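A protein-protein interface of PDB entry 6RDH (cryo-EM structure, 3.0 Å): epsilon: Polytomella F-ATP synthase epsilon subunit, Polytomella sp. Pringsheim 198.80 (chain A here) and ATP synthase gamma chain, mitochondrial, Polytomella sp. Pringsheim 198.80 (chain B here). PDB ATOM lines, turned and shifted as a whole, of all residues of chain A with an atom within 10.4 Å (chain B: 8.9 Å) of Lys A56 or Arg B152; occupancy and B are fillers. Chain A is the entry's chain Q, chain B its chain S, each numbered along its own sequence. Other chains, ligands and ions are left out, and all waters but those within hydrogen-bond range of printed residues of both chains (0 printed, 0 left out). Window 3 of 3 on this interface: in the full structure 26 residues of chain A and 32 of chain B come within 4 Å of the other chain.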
ATOM      1  N   ALA A  50      20.241 -10.929  17.561  1.00  0.00           N
ATOM      2  CA  ALA A  50      21.254 -10.580  18.542  1.00  0.00           C
ATOM      3  C   ALA A  50      20.646 -10.514  19.935  1.00  0.00           C
ATOM      4  O   ALA A  50      19.689  -9.762  20.152  1.00  0.00           O
ATOM      5  CB  ALA A  50      21.885  -9.237  18.182  1.00  0.00           C
ATOM      6  N   PRO A  51      21.156 -11.271  20.900  1.00  0.00           N
ATOM      7  CA  PRO A  51      20.617 -11.201  22.258  1.00  0.00           C
ATOM      8  C   PRO A  51      21.055  -9.930  22.963  1.00  0.00           C
ATOM      9  O   PRO A  51      22.034  -9.289  22.594  1.00  0.00           O
ATOM     10  CB  PRO A  51      21.210 -12.436  22.943  1.00  0.00           C
ATOM     11  CG  PRO A  51      21.745 -13.288  21.833  1.00  0.00           C
ATOM     12  CD  PRO A  51      22.149 -12.346  20.770  1.00  0.00           C
ATOM     13  N   TYR A  52      20.301  -9.567  23.998  1.00  0.00           N
ATOM     14  CA  TYR A  52      20.577  -8.366  24.788  1.00  0.00           C
ATOM     15  C   TYR A  52      20.612  -8.765  26.257  1.00  0.00           C
ATOM     16  O   TYR A  52      19.590  -8.737  26.945  1.00  0.00           O
ATOM     17  CB  TYR A  52      19.542  -7.289  24.524  1.00  0.00           C
ATOM     18  CG  TYR A  52      19.951  -6.315  23.452  1.00  0.00           C
ATOM     19  CD1 TYR A  52      20.163  -4.978  23.748  1.00  0.00           C
ATOM     20  CD2 TYR A  52      20.131  -6.733  22.142  1.00  0.00           C
ATOM     21  CE1 TYR A  52      20.541  -4.083  22.766  1.00  0.00           C
ATOM     22  CE2 TYR A  52      20.513  -5.851  21.154  1.00  0.00           C
ATOM     23  CZ  TYR A  52      20.714  -4.529  21.472  1.00  0.00           C
ATOM     24  OH  TYR A  52      21.086  -3.644  20.491  1.00  0.00           O
ATOM     25  N   VAL A  53      21.797  -9.111  26.743  1.00  0.00           N
ATOM     26  CA  VAL A  53      21.917  -9.651  28.090  1.00  0.00           C
ATOM     27  C   VAL A  53      22.087  -8.559  29.140  1.00  0.00           C
ATOM     28  O   VAL A  53      21.737  -8.767  30.304  1.00  0.00           O
ATOM     29  CB  VAL A  53      23.069 -10.668  28.146  1.00  0.00           C
ATOM     30  CG1 VAL A  53      22.738 -11.872  27.286  1.00  0.00           C
ATOM     31  CG2 VAL A  53      24.373 -10.039  27.668  1.00  0.00           C
ATOM     32  N   ASP A  54      22.608  -7.394  28.759  1.00  0.00           N
ATOM     33  CA  ASP A  54      22.868  -6.333  29.717  1.00  0.00           C
ATOM     34  C   ASP A  54      21.976  -5.118  29.538  1.00  0.00           C
ATOM     35  O   ASP A  54      21.626  -4.478  30.534  1.00  0.00           O
ATOM     36  CB  ASP A  54      24.337  -5.888  29.632  1.00  0.00           C
ATOM     37  CG  ASP A  54      24.706  -5.335  28.265  1.00  0.00           C
ATOM     38  OD1 ASP A  54      25.681  -4.561  28.187  1.00  0.00           O
ATOM     39  OD2 ASP A  54      24.018  -5.667  27.276  1.00  0.00           O
ATOM     40  N   GLY A  55      21.580  -4.810  28.310  1.00  0.00           N
ATOM     41  CA  GLY A  55      20.911  -3.563  28.027  1.00  0.00           C
ATOM     42  C   GLY A  55      21.427  -2.904  26.769  1.00  0.00           C
ATOM     43  O   GLY A  55      20.663  -2.227  26.081  1.00  0.00           O
ATOM     44  N   LYS A  56      22.705  -3.082  26.439  1.00  0.00           N
ATOM     45  CA  LYS A  56      23.224  -2.483  25.212  1.00  0.00           C
ATOM     46  C   LYS A  56      24.104  -3.437  24.415  1.00  0.00           C
ATOM     47  O   LYS A  56      24.275  -3.256  23.207  1.00  0.00           O
ATOM     48  CB  LYS A  56      24.003  -1.200  25.519  1.00  0.00           C
ATOM     49  CG  LYS A  56      23.129   0.018  25.801  1.00  0.00           C
ATOM     50  CD  LYS A  56      22.779   0.790  24.538  1.00  0.00           C
ATOM     51  CE  LYS A  56      22.828   2.297  24.786  1.00  0.00           C
ATOM     52  NZ  LYS A  56      22.408   3.107  23.606  1.00  0.00           N
ATOM     53  N   ALA A  57      24.682  -4.437  25.069  1.00  0.00           N
ATOM     54  CA  ALA A  57      25.607  -5.315  24.373  1.00  0.00           C
ATOM     55  C   ALA A  57      24.909  -6.572  23.868  1.00  0.00           C
ATOM     56  O   ALA A  57      23.799  -6.915  24.283  1.00  0.00           O
ATOM     57  CB  ALA A  57      26.773  -5.702  25.282  1.00  0.00           C
ATOM     58  N   GLY A  58      25.585  -7.260  22.952  1.00  0.00           N
ATOM     59  CA  GLY A  58      25.197  -8.597  22.552  1.00  0.00           C
ATOM     60  C   GLY A  58      25.896  -9.077  21.300  1.00  0.00           C
ATOM     61  O   GLY A  58      26.174  -8.282  20.399  1.00  0.00           O
ATOM     62  N   ALA A  59      26.173 -10.377  21.224  1.00  0.00           N
ATOM     63  CA  ALA A  59      26.767 -10.970  20.036  1.00  0.00           C
ATOM     64  C   ALA A  59      25.712 -11.079  18.943  1.00  0.00           C
ATOM     65  O   ALA A  59      24.529 -10.841  19.169  1.00  0.00           O
ATOM     66  CB  ALA A  59      27.362 -12.336  20.361  1.00  0.00           C
ATOM     67  N   SER A  60      26.121 -11.469  17.742  1.00  0.00           N
ATOM     68  CA  SER A  60      25.211 -11.441  16.610  1.00  0.00           C
ATOM     69  C   SER A  60      25.022 -12.835  16.037  1.00  0.00           C
ATOM     70  O   SER A  60      25.728 -13.783  16.385  1.00  0.00           O
ATOM     71  CB  SER A  60      25.703 -10.497  15.510  1.00  0.00           C
ATOM     72  OG  SER A  60      25.096 -10.818  14.271  1.00  0.00           O
ATOM     73  N   THR B 120       5.953   1.852  20.363  1.00  0.00           N
ATOM     74  CA  THR B 120       6.692   1.800  21.619  1.00  0.00           C
ATOM     75  C   THR B 120       5.841   2.324  22.768  1.00  0.00           C
ATOM     76  O   THR B 120       5.873   1.770  23.879  1.00  0.00           O
ATOM     77  CB  THR B 120       7.991   2.585  21.494  1.00  0.00           C
ATOM     78  OG1 THR B 120       8.680   2.151  20.320  1.00  0.00           O
ATOM     79  CG2 THR B 120       8.886   2.317  22.679  1.00  0.00           C
ATOM     80  N   ARG B 124       4.771  -0.141  25.967  1.00  0.00           N
ATOM     81  CA  ARG B 124       4.819   0.092  27.406  1.00  0.00           C
ATOM     82  C   ARG B 124       3.426   0.243  28.008  1.00  0.00           C
ATOM     83  O   ARG B 124       3.228  -0.102  29.174  1.00  0.00           O
ATOM     84  CB  ARG B 124       5.689   1.302  27.737  1.00  0.00           C
ATOM     85  CG  ARG B 124       5.292   2.578  27.060  1.00  0.00           C
ATOM     86  CD  ARG B 124       6.396   3.603  27.213  1.00  0.00           C
ATOM     87  NE  ARG B 124       6.446   4.161  28.557  1.00  0.00           N
ATOM     88  CZ  ARG B 124       6.175   5.429  28.838  1.00  0.00           C
ATOM     89  NH1 ARG B 124       5.844   6.267  27.867  1.00  0.00           N
ATOM     90  NH2 ARG B 124       6.237   5.861  30.088  1.00  0.00           N
ATOM     91  N   LYS B 145      14.425  -0.363  14.431  1.00  0.00           N
ATOM     92  CA  LYS B 145      13.878   0.774  15.150  1.00  0.00           C
ATOM     93  C   LYS B 145      13.215   0.388  16.463  1.00  0.00           C
ATOM     94  O   LYS B 145      12.639   1.253  17.127  1.00  0.00           O
ATOM     95  CB  LYS B 145      12.882   1.520  14.267  1.00  0.00           C
ATOM     96  CG  LYS B 145      13.501   2.141  13.041  1.00  0.00           C
ATOM     97  CD  LYS B 145      14.609   3.092  13.424  1.00  0.00           C
ATOM     98  CE  LYS B 145      15.450   3.460  12.221  1.00  0.00           C
ATOM     99  NZ  LYS B 145      16.667   4.215  12.603  1.00  0.00           N
ATOM    100  N   GLY B 146      13.280  -0.878  16.854  1.00  0.00           N
ATOM    101  CA  GLY B 146      12.771  -1.301  18.138  1.00  0.00           C
ATOM    102  C   GLY B 146      13.853  -1.301  19.192  1.00  0.00           C
ATOM    103  O   GLY B 146      13.619  -0.857  20.317  1.00  0.00           O
ATOM    104  N   ARG B 147      15.055  -1.765  18.836  1.00  0.00           N
ATOM    105  CA  ARG B 147      16.162  -1.751  19.785  1.00  0.00           C
ATOM    106  C   ARG B 147      16.667  -0.345  20.059  1.00  0.00           C
ATOM    107  O   ARG B 147      17.394  -0.138  21.035  1.00  0.00           O
ATOM    108  CB  ARG B 147      17.323  -2.607  19.285  1.00  0.00           C
ATOM    109  CG  ARG B 147      17.887  -2.168  17.963  1.00  0.00           C
ATOM    110  CD  ARG B 147      19.375  -2.424  17.888  1.00  0.00           C
ATOM    111  NE  ARG B 147      19.964  -1.807  16.708  1.00  0.00           N
ATOM    112  CZ  ARG B 147      20.352  -0.538  16.643  1.00  0.00           C
ATOM    113  NH1 ARG B 147      20.878  -0.063  15.524  1.00  0.00           N
ATOM    114  NH2 ARG B 147      20.214   0.261  17.691  1.00  0.00           N
ATOM    115  N   SER B 148      16.305   0.619  19.221  1.00  0.00           N
ATOM    116  CA  SER B 148      16.643   2.001  19.485  1.00  0.00           C
ATOM    117  C   SER B 148      15.749   2.634  20.537  1.00  0.00           C
ATOM    118  O   SER B 148      16.144   3.637  21.136  1.00  0.00           O
ATOM    119  CB  SER B 148      16.557   2.808  18.192  1.00  0.00           C
ATOM    120  OG  SER B 148      16.828   4.173  18.434  1.00  0.00           O
ATOM    121  N   GLN B 149      14.562   2.089  20.774  1.00  0.00           N
ATOM    122  CA  GLN B 149      13.608   2.723  21.674  1.00  0.00           C
ATOM    123  C   GLN B 149      13.147   1.838  22.816  1.00  0.00           C
ATOM    124  O   GLN B 149      12.831   2.359  23.889  1.00  0.00           O
ATOM    125  CB  GLN B 149      12.374   3.204  20.899  1.00  0.00           C
ATOM    126  CG  GLN B 149      12.700   4.094  19.733  1.00  0.00           C
ATOM    127  CD  GLN B 149      11.502   4.414  18.894  1.00  0.00           C
ATOM    128  OE1 GLN B 149      10.398   4.580  19.404  1.00  0.00           O
ATOM    129  NE2 GLN B 149      11.708   4.500  17.587  1.00  0.00           N
ATOM    130  N   LEU B 150      13.087   0.522  22.621  1.00  0.00           N
ATOM    131  CA  LEU B 150      12.736  -0.356  23.729  1.00  0.00           C
ATOM    132  C   LEU B 150      13.856  -0.417  24.751  1.00  0.00           C
ATOM    133  O   LEU B 150      13.594  -0.621  25.939  1.00  0.00           O
ATOM    134  CB  LEU B 150      12.402  -1.750  23.213  1.00  0.00           C
ATOM    135  CG  LEU B 150      11.109  -1.837  22.412  1.00  0.00           C
ATOM    136  CD1 LEU B 150      10.946  -3.221  21.879  1.00  0.00           C
ATOM    137  CD2 LEU B 150       9.917  -1.464  23.259  1.00  0.00           C
ATOM    138  N   THR B 151      15.100  -0.234  24.306  1.00  0.00           N
ATOM    139  CA  THR B 151      16.203   0.015  25.226  1.00  0.00           C
ATOM    140  C   THR B 151      15.984   1.304  26.013  1.00  0.00           C
ATOM    141  O   THR B 151      16.282   1.370  27.211  1.00  0.00           O
ATOM    142  CB  THR B 151      17.509   0.075  24.439  1.00  0.00           C
ATOM    143  OG1 THR B 151      17.666  -1.128  23.678  1.00  0.00           O
ATOM    144  CG2 THR B 151      18.694   0.247  25.360  1.00  0.00           C
ATOM    145  N   ARG B 152      15.432   2.331  25.364  1.00  0.00           N
ATOM    146  CA  ARG B 152      15.153   3.582  26.061  1.00  0.00           C
ATOM    147  C   ARG B 152      14.005   3.440  27.051  1.00  0.00           C
ATOM    148  O   ARG B 152      13.940   4.197  28.025  1.00  0.00           O
ATOM    149  CB  ARG B 152      14.838   4.699  25.064  1.00  0.00           C
ATOM    150  CG  ARG B 152      15.979   5.074  24.141  1.00  0.00           C
ATOM    151  CD  ARG B 152      16.857   6.158  24.734  1.00  0.00           C
ATOM    152  NE  ARG B 152      17.829   5.628  25.686  1.00  0.00           N
ATOM    153  CZ  ARG B 152      18.989   5.071  25.348  1.00  0.00           C
ATOM    154  NH1 ARG B 152      19.805   4.618  26.290  1.00  0.00           N
ATOM    155  NH2 ARG B 152      19.334   4.961  24.072  1.00  0.00           N
ATOM    156  N   ILE B 153      13.093   2.503  26.827  1.00  0.00           N
ATOM    157  CA  ILE B 153      12.001   2.263  27.765  1.00  0.00           C
ATOM    158  C   ILE B 153      12.341   1.151  28.748  1.00  0.00           C
ATOM    159  O   ILE B 153      12.451   1.390  29.950  1.00  0.00           O
ATOM    160  CB  ILE B 153      10.687   1.963  27.013  1.00  0.00           C
ATOM    161  CG1 ILE B 153      10.309   3.130  26.099  1.00  0.00           C
ATOM    162  CG2 ILE B 153       9.569   1.711  28.000  1.00  0.00           C
ATOM    163  CD1 ILE B 153      10.040   4.434  26.827  1.00  0.00           C
ATOM    164  N   GLU B 154      12.535  -0.069  28.256  1.00  0.00           N
ATOM    165  CA  GLU B 154      12.751  -1.244  29.098  1.00  0.00           C
ATOM    166  C   GLU B 154      14.160  -1.751  28.825  1.00  0.00           C
ATOM    167  O   GLU B 154      14.348  -2.652  28.010  1.00  0.00           O
ATOM    168  CB  GLU B 154      11.721  -2.315  28.800  1.00  0.00           C
ATOM    169  CG  GLU B 154      10.289  -1.846  28.880  1.00  0.00           C
ATOM    170  CD  GLU B 154       9.837  -1.605  30.300  1.00  0.00           C
ATOM    171  OE1 GLU B 154      10.298  -2.337  31.200  1.00  0.00           O
ATOM    172  OE2 GLU B 154       9.024  -0.686  30.521  1.00  0.00           O
ATOM    173  N   SER B 155      15.146  -1.187  29.519  1.00  0.00           N
ATOM    174  CA  SER B 155      16.534  -1.502  29.202  1.00  0.00           C
ATOM    175  C   SER B 155      16.950  -2.853  29.759  1.00  0.00           C
ATOM    176  O   SER B 155      17.809  -3.526  29.178  1.00  0.00           O
ATOM    177  CB  SER B 155      17.455  -0.410  29.740  1.00  0.00           C
ATOM    178  OG  SER B 155      18.785  -0.598  29.284  1.00  0.00           O
ATOM    179  N   GLN B 156      16.360  -3.264  30.878  1.00  0.00           N
ATOM    180  CA  GLN B 156      16.759  -4.493  31.548  1.00  0.00           C
ATOM    181  C   GLN B 156      15.983  -5.709  31.077  1.00  0.00           C
ATOM    182  O   GLN B 156      16.559  -6.796  30.976  1.00  0.00           O
ATOM    183  CB  GLN B 156      16.590  -4.345  33.062  1.00  0.00           C
ATOM    184  CG  GLN B 156      15.322  -3.630  33.470  1.00  0.00           C
ATOM    185  CD  GLN B 156      15.344  -3.196  34.919  1.00  0.00           C
ATOM    186  OE1 GLN B 156      16.403  -2.921  35.477  1.00  0.00           O
ATOM    187  NE2 GLN B 156      14.173  -3.132  35.536  1.00  0.00           N
ATOM    188  N   TYR B 158      14.687  -5.977  28.072  1.00  0.00           N
ATOM    189  CA  TYR B 158      14.981  -6.192  26.664  1.00  0.00           C
ATOM    190  C   TYR B 158      16.031  -7.277  26.529  1.00  0.00           C
ATOM    191  O   TYR B 158      17.091  -7.201  27.152  1.00  0.00           O
ATOM    192  CB  TYR B 158      15.474  -4.905  26.015  1.00  0.00           C
ATOM    193  CG  TYR B 158      15.505  -4.969  24.522  1.00  0.00           C
ATOM    194  CD1 TYR B 158      16.673  -5.279  23.852  1.00  0.00           C
ATOM    195  CD2 TYR B 158      14.368  -4.725  23.781  1.00  0.00           C
ATOM    196  CE1 TYR B 158      16.709  -5.346  22.486  1.00  0.00           C
ATOM    197  CE2 TYR B 158      14.394  -4.789  22.415  1.00  0.00           C
ATOM    198  CZ  TYR B 158      15.568  -5.101  21.778  1.00  0.00           C
ATOM    199  OH  TYR B 158      15.607  -5.166  20.416  1.00  0.00           O
ATOM    200  N   GLN B 159      15.736  -8.299  25.731  1.00  0.00           N
ATOM    201  CA  GLN B 159      16.600  -9.468  25.665  1.00  0.00           C
ATOM    202  C   GLN B 159      16.964  -9.922  24.262  1.00  0.00           C
ATOM    203  O   GLN B 159      17.960 -10.636  24.122  1.00  0.00           O
ATOM    204  CB  GLN B 159      15.960 -10.651  26.407  1.00  0.00           C
ATOM    205  CG  GLN B 159      15.736 -10.412  27.892  1.00  0.00           C
ATOM    206  CD  GLN B 159      15.286 -11.639  28.628  1.00  0.00           C
ATOM    207  OE1 GLN B 159      15.674 -12.751  28.287  1.00  0.00           O
ATOM    208  NE2 GLN B 159      14.465 -11.446  29.651  1.00  0.00           N
ATOM    209  N   ALA B 161      16.909  -8.982  19.768  1.00  0.00           N
ATOM    210  CA  ALA B 161      16.769  -7.975  18.720  1.00  0.00           C
ATOM    211  C   ALA B 161      16.839  -8.652  17.363  1.00  0.00           C
ATOM    212  O   ALA B 161      17.931  -8.968  16.889  1.00  0.00           O
ATOM    213  CB  ALA B 161      17.859  -6.914  18.833  1.00  0.00           C
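Among the printed residues, merely in contact across the chains: Pro A51 with Gln B159, Tyr A52 with Arg B147, Tyr A52 with Ala B161, Gly A55 with Thr B151, Gly A55 with Ser B155 and Lys A56 with Arg B152.
Of the 11 printed residues of chain A, 5 touch a printed residue of chain B.
Hydrophobic or aromatic side chains of chain A within 4 Å of the printed part of chain B: Pro A51 and Tyr A52.
Along chain A the printed residues that touch a printed residue of chain B span positions 50 to 56.
Printed residues of chain B that touch a printed residue of chain A: Arg B147, Thr B151, Arg B152, Ser B155, Tyr B158, Gln B159 and Ala B161.
Hydrophobic or aromatic side chains of chain B that line the printed part of chain A: Tyr B158 and Ala B161.
Among the printed residues, 9 pairs touch across the chains.
Of the printed residues of chain B, Pro A51 touches Gln B159.
Of chain B, only Arg B152 (3.6 Å) comes within 4 Å of Lys A56.
No residue of chain B comes within 4 Å of Ala A57.
Printed residues of chain A within 4 Å of Arg B147: Tyr A52 (3.3 Å).
Thr B151 touches one residue of chain A.
Of chain A, only Lys A56 (3.6 Å) comes within 4 Å of Arg B152.
No residue of chain A comes within 4 Å of Ile B153.
Glu B154 touches none of the printed residues of chain A.
Of the printed residues of chain A, Tyr B158 touches Tyr A52 (2.9 Å).
Of the printed residues of chain A, Gln B159 touches Pro A51 and Tyr A52.
The backbone NH (N) of Ala B161 sits at hydrogen-bond distance from the backbone carbonyl oxygen (O) of Ala A50 (2.9 Å).
The backbone NH of Tyr A52 sits at hydrogen-bond distance from the backbone carbonyl oxygen of Gln B159 (2.6 Å).
The backbone carbonyl oxygen (O) of Tyr A52 sits close to the backbone carbonyl oxygen (O) of Tyr B158 (2.9 Å).
N of Lys A56 is in hydrogen-bond range of OD2 of Asp A54 (3.0 Å).
The backbone carbonyl oxygen of Arg B147 lies within hydrogen-bond range of the side-chain hydroxyl of Thr B151 (2.8 Å).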
